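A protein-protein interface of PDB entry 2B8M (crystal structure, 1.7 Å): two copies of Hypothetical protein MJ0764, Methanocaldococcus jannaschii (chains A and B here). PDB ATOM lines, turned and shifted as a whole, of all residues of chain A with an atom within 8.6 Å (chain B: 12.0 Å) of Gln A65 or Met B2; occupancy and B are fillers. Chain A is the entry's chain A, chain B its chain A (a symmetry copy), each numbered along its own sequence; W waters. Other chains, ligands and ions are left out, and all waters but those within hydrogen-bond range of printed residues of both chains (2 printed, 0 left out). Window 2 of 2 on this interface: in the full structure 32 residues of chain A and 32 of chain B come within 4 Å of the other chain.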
ATOM      1  N   LEU A  60     -12.553  -4.804  18.158  1.00  0.00           N
ATOM      2  CA  LEU A  60     -12.309  -5.089  16.752  1.00  0.00           C
ATOM      3  C   LEU A  60     -11.833  -3.818  16.052  1.00  0.00           C
ATOM      4  O   LEU A  60     -12.506  -2.809  16.043  1.00  0.00           O
ATOM      5  CB  LEU A  60     -13.621  -5.543  16.107  1.00  0.00           C
ATOM      6  CG  LEU A  60     -13.507  -5.893  14.630  1.00  0.00           C
ATOM      7  CD1 LEU A  60     -12.627  -7.107  14.437  1.00  0.00           C
ATOM      8  CD2 LEU A  60     -14.895  -6.134  14.042  1.00  0.00           C
ATOM      9  N   THR A  61     -10.619  -3.842  15.526  1.00  0.00           N
ATOM     10  CA  THR A  61     -10.088  -2.738  14.765  1.00  0.00           C
ATOM     11  C   THR A  61      -9.980  -3.164  13.314  1.00  0.00           C
ATOM     12  O   THR A  61      -9.279  -4.126  12.990  1.00  0.00           O
ATOM     13  CB  THR A  61      -8.707  -2.250  15.302  1.00  0.00           C
ATOM     14  OG1 THR A  61      -8.793  -2.047  16.730  1.00  0.00           O
ATOM     15  CG2 THR A  61      -8.347  -0.947  14.681  1.00  0.00           C
ATOM     16  N   LEU A  62     -10.675  -2.423  12.448  1.00  0.00           N
ATOM     17  CA  LEU A  62     -10.685  -2.673  11.045  1.00  0.00           C
ATOM     18  C   LEU A  62     -10.053  -1.502  10.323  1.00  0.00           C
ATOM     19  O   LEU A  62     -10.383  -0.324  10.575  1.00  0.00           O
ATOM     20  CB  LEU A  62     -12.102  -2.882  10.515  1.00  0.00           C
ATOM     21  CG  LEU A  62     -12.924  -4.014  11.104  1.00  0.00           C
ATOM     22  CD1 LEU A  62     -14.235  -4.085  10.344  1.00  0.00           C
ATOM     23  CD2 LEU A  62     -12.201  -5.345  11.035  1.00  0.00           C
ATOM     24  N   GLU A  63      -9.126  -1.820   9.434  1.00  0.00           N
ATOM     25  CA  GLU A  63      -8.440  -0.805   8.639  1.00  0.00           C
ATOM     26  C   GLU A  63      -8.020   0.398   9.469  1.00  0.00           C
ATOM     27  O   GLU A  63      -7.313   0.207  10.436  1.00  0.00           O
ATOM     28  CB  GLU A  63      -9.269  -0.414   7.411  1.00  0.00           C
ATOM     29  CG  GLU A  63      -9.500  -1.505   6.420  1.00  0.00           C
ATOM     30  CD  GLU A  63      -8.263  -1.930   5.622  1.00  0.00           C
ATOM     31  OE1 GLU A  63      -7.300  -1.150   5.509  1.00  0.00           O
ATOM     32  OE2 GLU A  63      -8.249  -3.066   5.074  1.00  0.00           O
ATOM     33  N   ASP A  64      -8.441   1.603   9.087  1.00  0.00           N
ATOM     34  CA  ASP A  64      -8.043   2.871   9.745  1.00  0.00           C
ATOM     35  C   ASP A  64      -9.059   3.375  10.767  1.00  0.00           C
ATOM     36  O   ASP A  64      -8.938   4.510  11.271  1.00  0.00           O
ATOM     37  CB  ASP A  64      -7.782   3.945   8.675  1.00  0.00           C
ATOM     38  CG  ASP A  64      -6.469   3.707   7.927  1.00  0.00           C
ATOM     39  N   GLN A  65     -10.046   2.541  11.081  1.00  0.00           N
ATOM     40  CA  GLN A  65     -11.079   2.894  12.051  1.00  0.00           C
ATOM     41  C   GLN A  65     -10.527   2.860  13.464  1.00  0.00           C
ATOM     42  O   GLN A  65      -9.577   2.137  13.765  1.00  0.00           O
ATOM     43  CB  GLN A  65     -12.235   1.889  12.015  1.00  0.00           C
ATOM     44  CG  GLN A  65     -12.937   1.728  10.680  1.00  0.00           C
ATOM     45  CD  GLN A  65     -14.238   0.940  10.748  1.00  0.00           C
ATOM     46  OE1 GLN A  65     -14.441   0.042  11.592  1.00  0.00           O
ATOM     47  NE2 GLN A  65     -15.119   1.248   9.834  1.00  0.00           N
ATOM     48  N   GLU A  66     -11.163   3.637  14.335  1.00  0.00           N
ATOM     49  CA  GLU A  66     -11.007   3.448  15.773  1.00  0.00           C
ATOM     50  C   GLU A  66     -11.493   2.039  16.162  1.00  0.00           C
ATOM     51  O   GLU A  66     -12.304   1.419  15.467  1.00  0.00           O
ATOM     52  CB  GLU A  66     -11.773   4.515  16.549  1.00  0.00           C
ATOM     53  CG  GLU A  66     -11.292   5.938  16.252  1.00  0.00           C
ATOM     54  CD  GLU A  66      -9.801   6.121  16.494  1.00  0.00           C
ATOM     55  OE1 GLU A  66      -9.298   5.669  17.554  1.00  0.00           O
ATOM     56  OE2 GLU A  66      -9.128   6.707  15.614  1.00  0.00           O
ATOM     57  N   PRO A  67     -10.948   1.508  17.261  1.00  0.00           N
ATOM     58  CA  PRO A  67     -11.396   0.209  17.715  1.00  0.00           C
ATOM     59  C   PRO A  67     -12.874   0.268  18.081  1.00  0.00           C
ATOM     60  O   PRO A  67     -13.314   1.257  18.670  1.00  0.00           O
ATOM     61  CB  PRO A  67     -10.541  -0.046  18.962  1.00  0.00           C
ATOM     62  CG  PRO A  67      -9.923   1.249  19.301  1.00  0.00           C
ATOM     63  CD  PRO A  67      -9.859   2.057  18.086  1.00  0.00           C
ATOM     64  N   HIS A  68     -13.638  -0.734  17.671  1.00  0.00           N
ATOM     65  CA  HIS A  68     -15.059  -0.805  18.033  1.00  0.00           C
ATOM     66  C   HIS A  68     -15.283  -1.991  18.965  1.00  0.00           C
ATOM     67  O   HIS A  68     -14.709  -3.064  18.733  1.00  0.00           O
ATOM     68  CB  HIS A  68     -15.935  -0.876  16.773  1.00  0.00           C
ATOM     69  CG  HIS A  68     -15.858   0.349  15.907  1.00  0.00           C
ATOM     70  ND1 HIS A  68     -16.133   0.318  14.557  1.00  0.00           N
ATOM     71  CD2 HIS A  68     -15.526   1.628  16.189  1.00  0.00           C
ATOM     72  CE1 HIS A  68     -15.978   1.525  14.047  1.00  0.00           C
ATOM     73  NE2 HIS A  68     -15.605   2.339  15.010  1.00  0.00           N
ATOM     74  N   ASN A  69     -16.098  -1.812  20.005  1.00  0.00           N
ATOM     75  CA  ASN A  69     -16.382  -2.891  20.953  1.00  0.00           C
ATOM     76  C   ASN A  69     -17.709  -3.565  20.695  1.00  0.00           C
ATOM     77  O   ASN A  69     -18.729  -2.912  20.489  1.00  0.00           O
ATOM     78  CB  ASN A  69     -16.351  -2.377  22.386  1.00  0.00           C
ATOM     79  CG  ASN A  69     -14.980  -1.824  22.775  1.00  0.00           C
ATOM     80  OD1 ASN A  69     -13.949  -2.388  22.441  1.00  0.00           O
ATOM     81  ND2 ASN A  69     -14.987  -0.740  23.516  1.00  0.00           N
ATOM     82  N   TYR A  70     -17.702  -4.895  20.705  1.00  0.00           N
ATOM     83  CA  TYR A  70     -18.923  -5.676  20.508  1.00  0.00           C
ATOM     84  C   TYR A  70     -19.019  -6.731  21.601  1.00  0.00           C
ATOM     85  O   TYR A  70     -18.054  -7.346  21.939  1.00  0.00           O
ATOM     86  CB  TYR A  70     -18.896  -6.331  19.132  1.00  0.00           C
ATOM     87  CG  TYR A  70     -18.927  -5.276  18.055  1.00  0.00           C
ATOM     88  CD1 TYR A  70     -20.090  -4.530  17.841  1.00  0.00           C
ATOM     89  CD2 TYR A  70     -17.811  -5.000  17.266  1.00  0.00           C
ATOM     90  CE1 TYR A  70     -20.134  -3.513  16.879  1.00  0.00           C
ATOM     91  CE2 TYR A  70     -17.852  -4.001  16.287  1.00  0.00           C
ATOM     92  CZ  TYR A  70     -19.021  -3.287  16.085  1.00  0.00           C
ATOM     93  OH  TYR A  70     -19.044  -2.285  15.159  1.00  0.00           O
ATOM     94  N   VAL A  76     -21.010  -9.982  14.017  1.00  0.00           N
ATOM     95  CA  VAL A  76     -20.345  -8.906  13.297  1.00  0.00           C
ATOM     96  C   VAL A  76     -19.813  -9.422  11.968  1.00  0.00           C
ATOM     97  O   VAL A  76     -19.011 -10.367  11.926  1.00  0.00           O
ATOM     98  CB  VAL A  76     -19.195  -8.285  14.113  1.00  0.00           C
ATOM     99  CG1 VAL A  76     -18.534  -7.130  13.299  1.00  0.00           C
ATOM    100  CG2 VAL A  76     -19.643  -7.812  15.469  1.00  0.00           C
ATOM    101  N   TYR A  77     -20.238  -8.783  10.883  1.00  0.00           N
ATOM    102  CA  TYR A  77     -19.765  -9.071   9.534  1.00  0.00           C
ATOM    103  C   TYR A  77     -18.516  -8.270   9.226  1.00  0.00           C
ATOM    104  O   TYR A  77     -18.510  -7.049   9.409  1.00  0.00           O
ATOM    105  CB  TYR A  77     -20.819  -8.667   8.516  1.00  0.00           C
ATOM    106  CG  TYR A  77     -20.348  -8.641   7.082  1.00  0.00           C
ATOM    107  CD1 TYR A  77     -19.875  -9.785   6.458  1.00  0.00           C
ATOM    108  CD2 TYR A  77     -20.393  -7.462   6.352  1.00  0.00           C
ATOM    109  CE1 TYR A  77     -19.482  -9.744   5.121  1.00  0.00           C
ATOM    110  CE2 TYR A  77     -20.010  -7.411   5.027  1.00  0.00           C
ATOM    111  CZ  TYR A  77     -19.563  -8.551   4.414  1.00  0.00           C
ATOM    112  OH  TYR A  77     -19.162  -8.453   3.098  1.00  0.00           O
ATOM    113  N   VAL A  78     -17.480  -8.944   8.745  1.00  0.00           N
ATOM    114  CA  VAL A  78     -16.283  -8.258   8.215  1.00  0.00           C
ATOM    115  C   VAL A  78     -16.148  -8.714   6.766  1.00  0.00           C
ATOM    116  O   VAL A  78     -16.077  -9.894   6.500  1.00  0.00           O
ATOM    117  CB  VAL A  78     -14.964  -8.599   8.956  1.00  0.00           C
ATOM    118  CG1 VAL A  78     -13.808  -7.818   8.350  1.00  0.00           C
ATOM    119  CG2 VAL A  78     -15.090  -8.324  10.433  1.00  0.00           C
ATOM    120  N   PRO A  79     -16.119  -7.774   5.830  1.00  0.00           N
ATOM    121  CA  PRO A  79     -15.937  -8.161   4.448  1.00  0.00           C
ATOM    122  C   PRO A  79     -14.589  -8.837   4.180  1.00  0.00           C
ATOM    123  O   PRO A  79     -13.617  -8.648   4.915  1.00  0.00           O
ATOM    124  CB  PRO A  79     -16.051  -6.816   3.690  1.00  0.00           C
ATOM    125  CG  PRO A  79     -16.692  -5.873   4.651  1.00  0.00           C
ATOM    126  CD  PRO A  79     -16.301  -6.322   5.995  1.00  0.00           C
ATOM    127  N   VAL A  82     -10.156  -7.310   4.158  1.00  0.00           N
ATOM    128  CA  VAL A  82     -10.170  -6.204   5.099  1.00  0.00           C
ATOM    129  C   VAL A  82      -9.160  -6.507   6.232  1.00  0.00           C
ATOM    130  O   VAL A  82      -9.185  -7.610   6.830  1.00  0.00           O
ATOM    131  CB  VAL A  82     -11.599  -6.011   5.697  1.00  0.00           C
ATOM    132  CG1 VAL A  82     -11.604  -5.035   6.870  1.00  0.00           C
ATOM    133  CG2 VAL A  82     -12.576  -5.527   4.648  1.00  0.00           C
ATOM    134  N   LYS A  83      -8.321  -5.529   6.555  1.00  0.00           N
ATOM    135  CA  LYS A  83      -7.358  -5.659   7.636  1.00  0.00           C
ATOM    136  C   LYS A  83      -8.065  -5.597   8.963  1.00  0.00           C
ATOM    137  O   LYS A  83      -8.807  -4.621   9.234  1.00  0.00           O
ATOM    138  CB  LYS A  83      -6.325  -4.557   7.585  1.00  0.00           C
ATOM    139  CG  LYS A  83      -5.215  -4.733   8.581  1.00  0.00           C
ATOM    140  CD  LYS A  83      -3.981  -3.934   8.213  1.00  0.00           C
ATOM    141  CE  LYS A  83      -4.262  -2.466   7.983  1.00  0.00           C
ATOM    142  NZ  LYS A  83      -3.047  -1.679   7.744  1.00  0.00           N
ATOM    143  N   GLY B   1     -20.245   5.441   6.928  1.00  0.00           N
ATOM    144  CA  GLY B   1     -20.607   4.302   7.787  1.00  0.00           C
ATOM    145  C   GLY B   1     -19.401   3.434   8.104  1.00  0.00           C
ATOM    146  O   GLY B   1     -18.286   3.709   7.677  1.00  0.00           O
ATOM    147  N   MET B   2     -19.640   2.370   8.838  1.00  0.00           N
ATOM    148  CA  MET B   2     -18.571   1.486   9.288  1.00  0.00           C
ATOM    149  C   MET B   2     -18.323   0.487   8.199  1.00  0.00           C
ATOM    150  O   MET B   2     -19.194   0.284   7.337  1.00  0.00           O
ATOM    151  CB  MET B   2     -19.043   0.742  10.531  1.00  0.00           C
ATOM    152  CG  MET B   2     -19.458   1.685  11.618  1.00  0.00           C
ATOM    153  SD  MET B   2     -19.796   0.631  13.178  1.00  0.00           S
ATOM    154  CE  MET B   2     -21.348  -0.428  12.599  1.00  0.00           C
ATOM    155  N   ILE B   3     -17.150  -0.152   8.236  1.00  0.00           N
ATOM    156  CA  ILE B   3     -16.844  -1.224   7.326  1.00  0.00           C
ATOM    157  C   ILE B   3     -17.672  -2.456   7.660  1.00  0.00           C
ATOM    158  O   ILE B   3     -18.151  -3.141   6.753  1.00  0.00           O
ATOM    159  CB  ILE B   3     -15.321  -1.541   7.397  1.00  0.00           C
ATOM    160  CG1 ILE B   3     -14.529  -0.382   6.757  1.00  0.00           C
ATOM    161  CG2 ILE B   3     -15.020  -2.929   6.835  1.00  0.00           C
ATOM    162  CD1 ILE B   3     -13.027  -0.370   7.080  1.00  0.00           C
ATOM    163  N   GLU B   4     -17.823  -2.725   8.959  1.00  0.00           N
ATOM    164  CA  GLU B   4     -18.534  -3.893   9.437  1.00  0.00           C
ATOM    165  C   GLU B   4     -20.025  -3.618   9.474  1.00  0.00           C
ATOM    166  O   GLU B   4     -20.450  -2.450   9.455  1.00  0.00           O
ATOM    167  CB  GLU B   4     -18.049  -4.319  10.826  1.00  0.00           C
ATOM    168  CG  GLU B   4     -18.381  -3.364  11.988  1.00  0.00           C
ATOM    169  CD  GLU B   4     -17.303  -2.338  12.311  1.00  0.00           C
ATOM    170  OE1 GLU B   4     -16.696  -1.765  11.391  1.00  0.00           O
ATOM    171  OE2 GLU B   4     -17.092  -2.048  13.510  1.00  0.00           O
ATOM    172  N   LYS B   5     -20.784  -4.714   9.493  1.00  0.00           N
ATOM    173  CA  LYS B   5     -22.223  -4.698   9.678  1.00  0.00           C
ATOM    174  C   LYS B   5     -22.521  -5.493  10.946  1.00  0.00           C
ATOM    175  O   LYS B   5     -21.909  -6.537  11.186  1.00  0.00           O
ATOM    176  CB  LYS B   5     -22.890  -5.306   8.436  1.00  0.00           C
ATOM    177  CG  LYS B   5     -24.391  -5.174   8.395  1.00  0.00           C
ATOM    178  CD  LYS B   5     -24.914  -5.302   6.954  1.00  0.00           C
ATOM    179  N   VAL B   6     -23.464  -5.002  11.745  1.00  0.00           N
ATOM    180  CA  VAL B   6     -23.735  -5.603  13.034  1.00  0.00           C
ATOM    181  C   VAL B   6     -25.173  -6.143  13.041  1.00  0.00           C
ATOM    182  O   VAL B   6     -26.086  -5.517  12.511  1.00  0.00           O
ATOM    183  CB  VAL B   6     -23.523  -4.557  14.141  1.00  0.00           C
ATOM    184  CG1 VAL B   6     -23.656  -5.181  15.510  1.00  0.00           C
ATOM    185  CG2 VAL B   6     -22.147  -3.954  14.011  1.00  0.00           C
ATOM    186  N   TYR B   7     -25.342  -7.302  13.673  1.00  0.00           N
ATOM    187  CA  TYR B   7     -26.618  -7.937  13.927  1.00  0.00           C
ATOM    188  C   TYR B   7     -26.665  -8.232  15.408  1.00  0.00           C
ATOM    189  O   TYR B   7     -25.627  -8.489  16.045  1.00  0.00           O
ATOM    190  CB  TYR B   7     -26.693  -9.290  13.202  1.00  0.00           C
ATOM    191  CG  TYR B   7     -26.492  -9.210  11.717  1.00  0.00           C
ATOM    192  CD1 TYR B   7     -25.207  -9.032  11.160  1.00  0.00           C
ATOM    193  CD2 TYR B   7     -27.590  -9.321  10.829  1.00  0.00           C
ATOM    194  CE1 TYR B   7     -25.032  -8.922   9.725  1.00  0.00           C
ATOM    195  CE2 TYR B   7     -27.418  -9.248   9.444  1.00  0.00           C
ATOM    196  CZ  TYR B   7     -26.143  -9.035   8.906  1.00  0.00           C
ATOM    197  OH  TYR B   7     -25.980  -8.992   7.536  1.00  0.00           O
ATOM    198  N   GLU B   8     -27.856  -8.280  15.962  1.00  0.00           N
ATOM    199  CA  GLU B   8     -28.011  -8.703  17.354  1.00  0.00           C
ATOM    200  C   GLU B   8     -28.942  -9.906  17.439  1.00  0.00           C
ATOM    201  O   GLU B   8     -29.922  -9.991  16.676  1.00  0.00           O
ATOM    202  CB  GLU B   8     -28.542  -7.575  18.242  1.00  0.00           C
ATOM    203  CG  GLU B   8     -27.662  -6.362  18.314  1.00  0.00           C
ATOM    204  CD  GLU B   8     -28.388  -5.158  18.832  1.00  0.00           C
ATOM    205  OE1 GLU B   8     -29.650  -5.172  18.863  1.00  0.00           O
ATOM    206  OE2 GLU B   8     -27.716  -4.177  19.253  1.00  0.00           O
HETATM  207  O   HOH W   1     -20.350  -0.319  16.368  1.00  0.00           O
HETATM  208  O   HOH W   2     -15.001   3.224   8.038  1.00  0.00           O
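Printed residues of chain A that touch a printed residue of chain B: Leu A62, Glu A63, Gln A65, His A68, Tyr A70, Val A76, Tyr A77 and Pro A79.
Hydrophobic or aromatic side chains of chain A that line the printed part of chain B: Leu A62, His A68, Tyr A70, Val A76, Tyr A77 and Pro A79.
Among the printed residues, no Asp or Glu carboxylate lies within 4 Å of a Lys or Arg side-chain nitrogen of the other chain.
No position is printed for both chains.
Of the 16 pairs that touch across the chains among the printed residues, none has its exchanged pair printed and touching as well.
The backbone NH (N) of Ile B3 lies close to the side-chain amide nitrogen (NE2) of Gln A65, 2.9 Å away.
The side-chain amide oxygen (OE1) of Gln A65 sits close to the side-chain carboxylate (OE1) of Glu B4 (2.9 Å).
OH of Tyr A70 sits at hydrogen-bond distance from OE2 of Glu B4 (2.6 Å).
OH of Tyr A70 lies within hydrogen-bond range of SD of Met B2 (3.6 Å).
The backbone NH of Tyr A77 is in hydrogen-bond range of the backbone carbonyl oxygen of Lys B5.
The side-chain carboxylate of Glu B4 is in hydrogen-bond range of a ring nitrogen (ND1) of His A68 (2.8 Å).
Water W1 lies within hydrogen-bond range of the side-chain hydroxyl of Tyr A70 (2.7 Å) and the side-chain sulfur of Met B2 (3.4 Å).
Water W2 lies within hydrogen-bond range of NE2 of Gln A65 and O of Gly B1.
Printed residues of chain B within 4 Å of Gln A65: Met B2, Ile B3 and Glu B4.
Of the printed residues of chain A, Met B2 touches Gln A65 (3.5 Å), His A68 (3.9 Å) and Tyr A70 (3.6 Å).
No residue of chain B comes within 4 Å of Thr A61.
Of chain B, only Ile B3 and Glu B4 come within 4 Å of Leu A62.
No residue of chain B comes within 4 Å of Asp A64.
Pro A67 touches none of the printed residues of chain B.
Printed residues of chain B within 4 Å of His A68: Met B2 and Glu B4.
No residue of chain A comes within 4 Å of Gly B1.
Printed residues of chain B within 4 Å of Val A76: Glu B4 (3.8 Å) and Lys B5 (3.5 Å).
Printed residues of chain A within 4 Å of Glu B4: Leu A62, Gln A65, His A68, Tyr A70, Val A76 and Tyr A77.
Of the printed residues of chain A, Ile B3 touches Leu A62, Glu A63, Gln A65 and Pro A79.
Printed residues of chain B within 4 Å of Tyr A77: Glu B4 (3.1 Å) and Lys B5 (2.8 Å).
The nearest residue of chain A that does not touch Met B2 is Leu A62 (6.5 Å).
Among the printed residues, pairs that only touch across the chains: Tyr A77 with Glu B4 (3.1 Å), Gln A65 with Met B2 (3.5 Å), Tyr A70 with Val B6 (3.5 Å), Val A76 with Lys B5 (3.5 Å), Leu A62 with Glu B4 (3.5 Å), Pro A79 with Ile B3 (3.7 Å), Glu A63 with Ile B3 (3.8 Å), Val A76 with Glu B4 (3.8 Å), Leu A62 with Ile B3 (3.8 Å) and His A68 with Met B2 (3.9 Å).
The backbone NH (N) of Leu A60 sits at hydrogen-bond distance from the backbone carbonyl oxygen (O) of His A68, 2.8 Å away.
O of Glu A66 lies close to NE2 of His A68.
ND1 of His A68 lies close to OE1 of Gln A65, at 3.4 Å.
The backbone NH (N) of Glu A63 is in hydrogen-bond range of the backbone carbonyl oxygen (O) of Lys A83 (2.8 Å).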
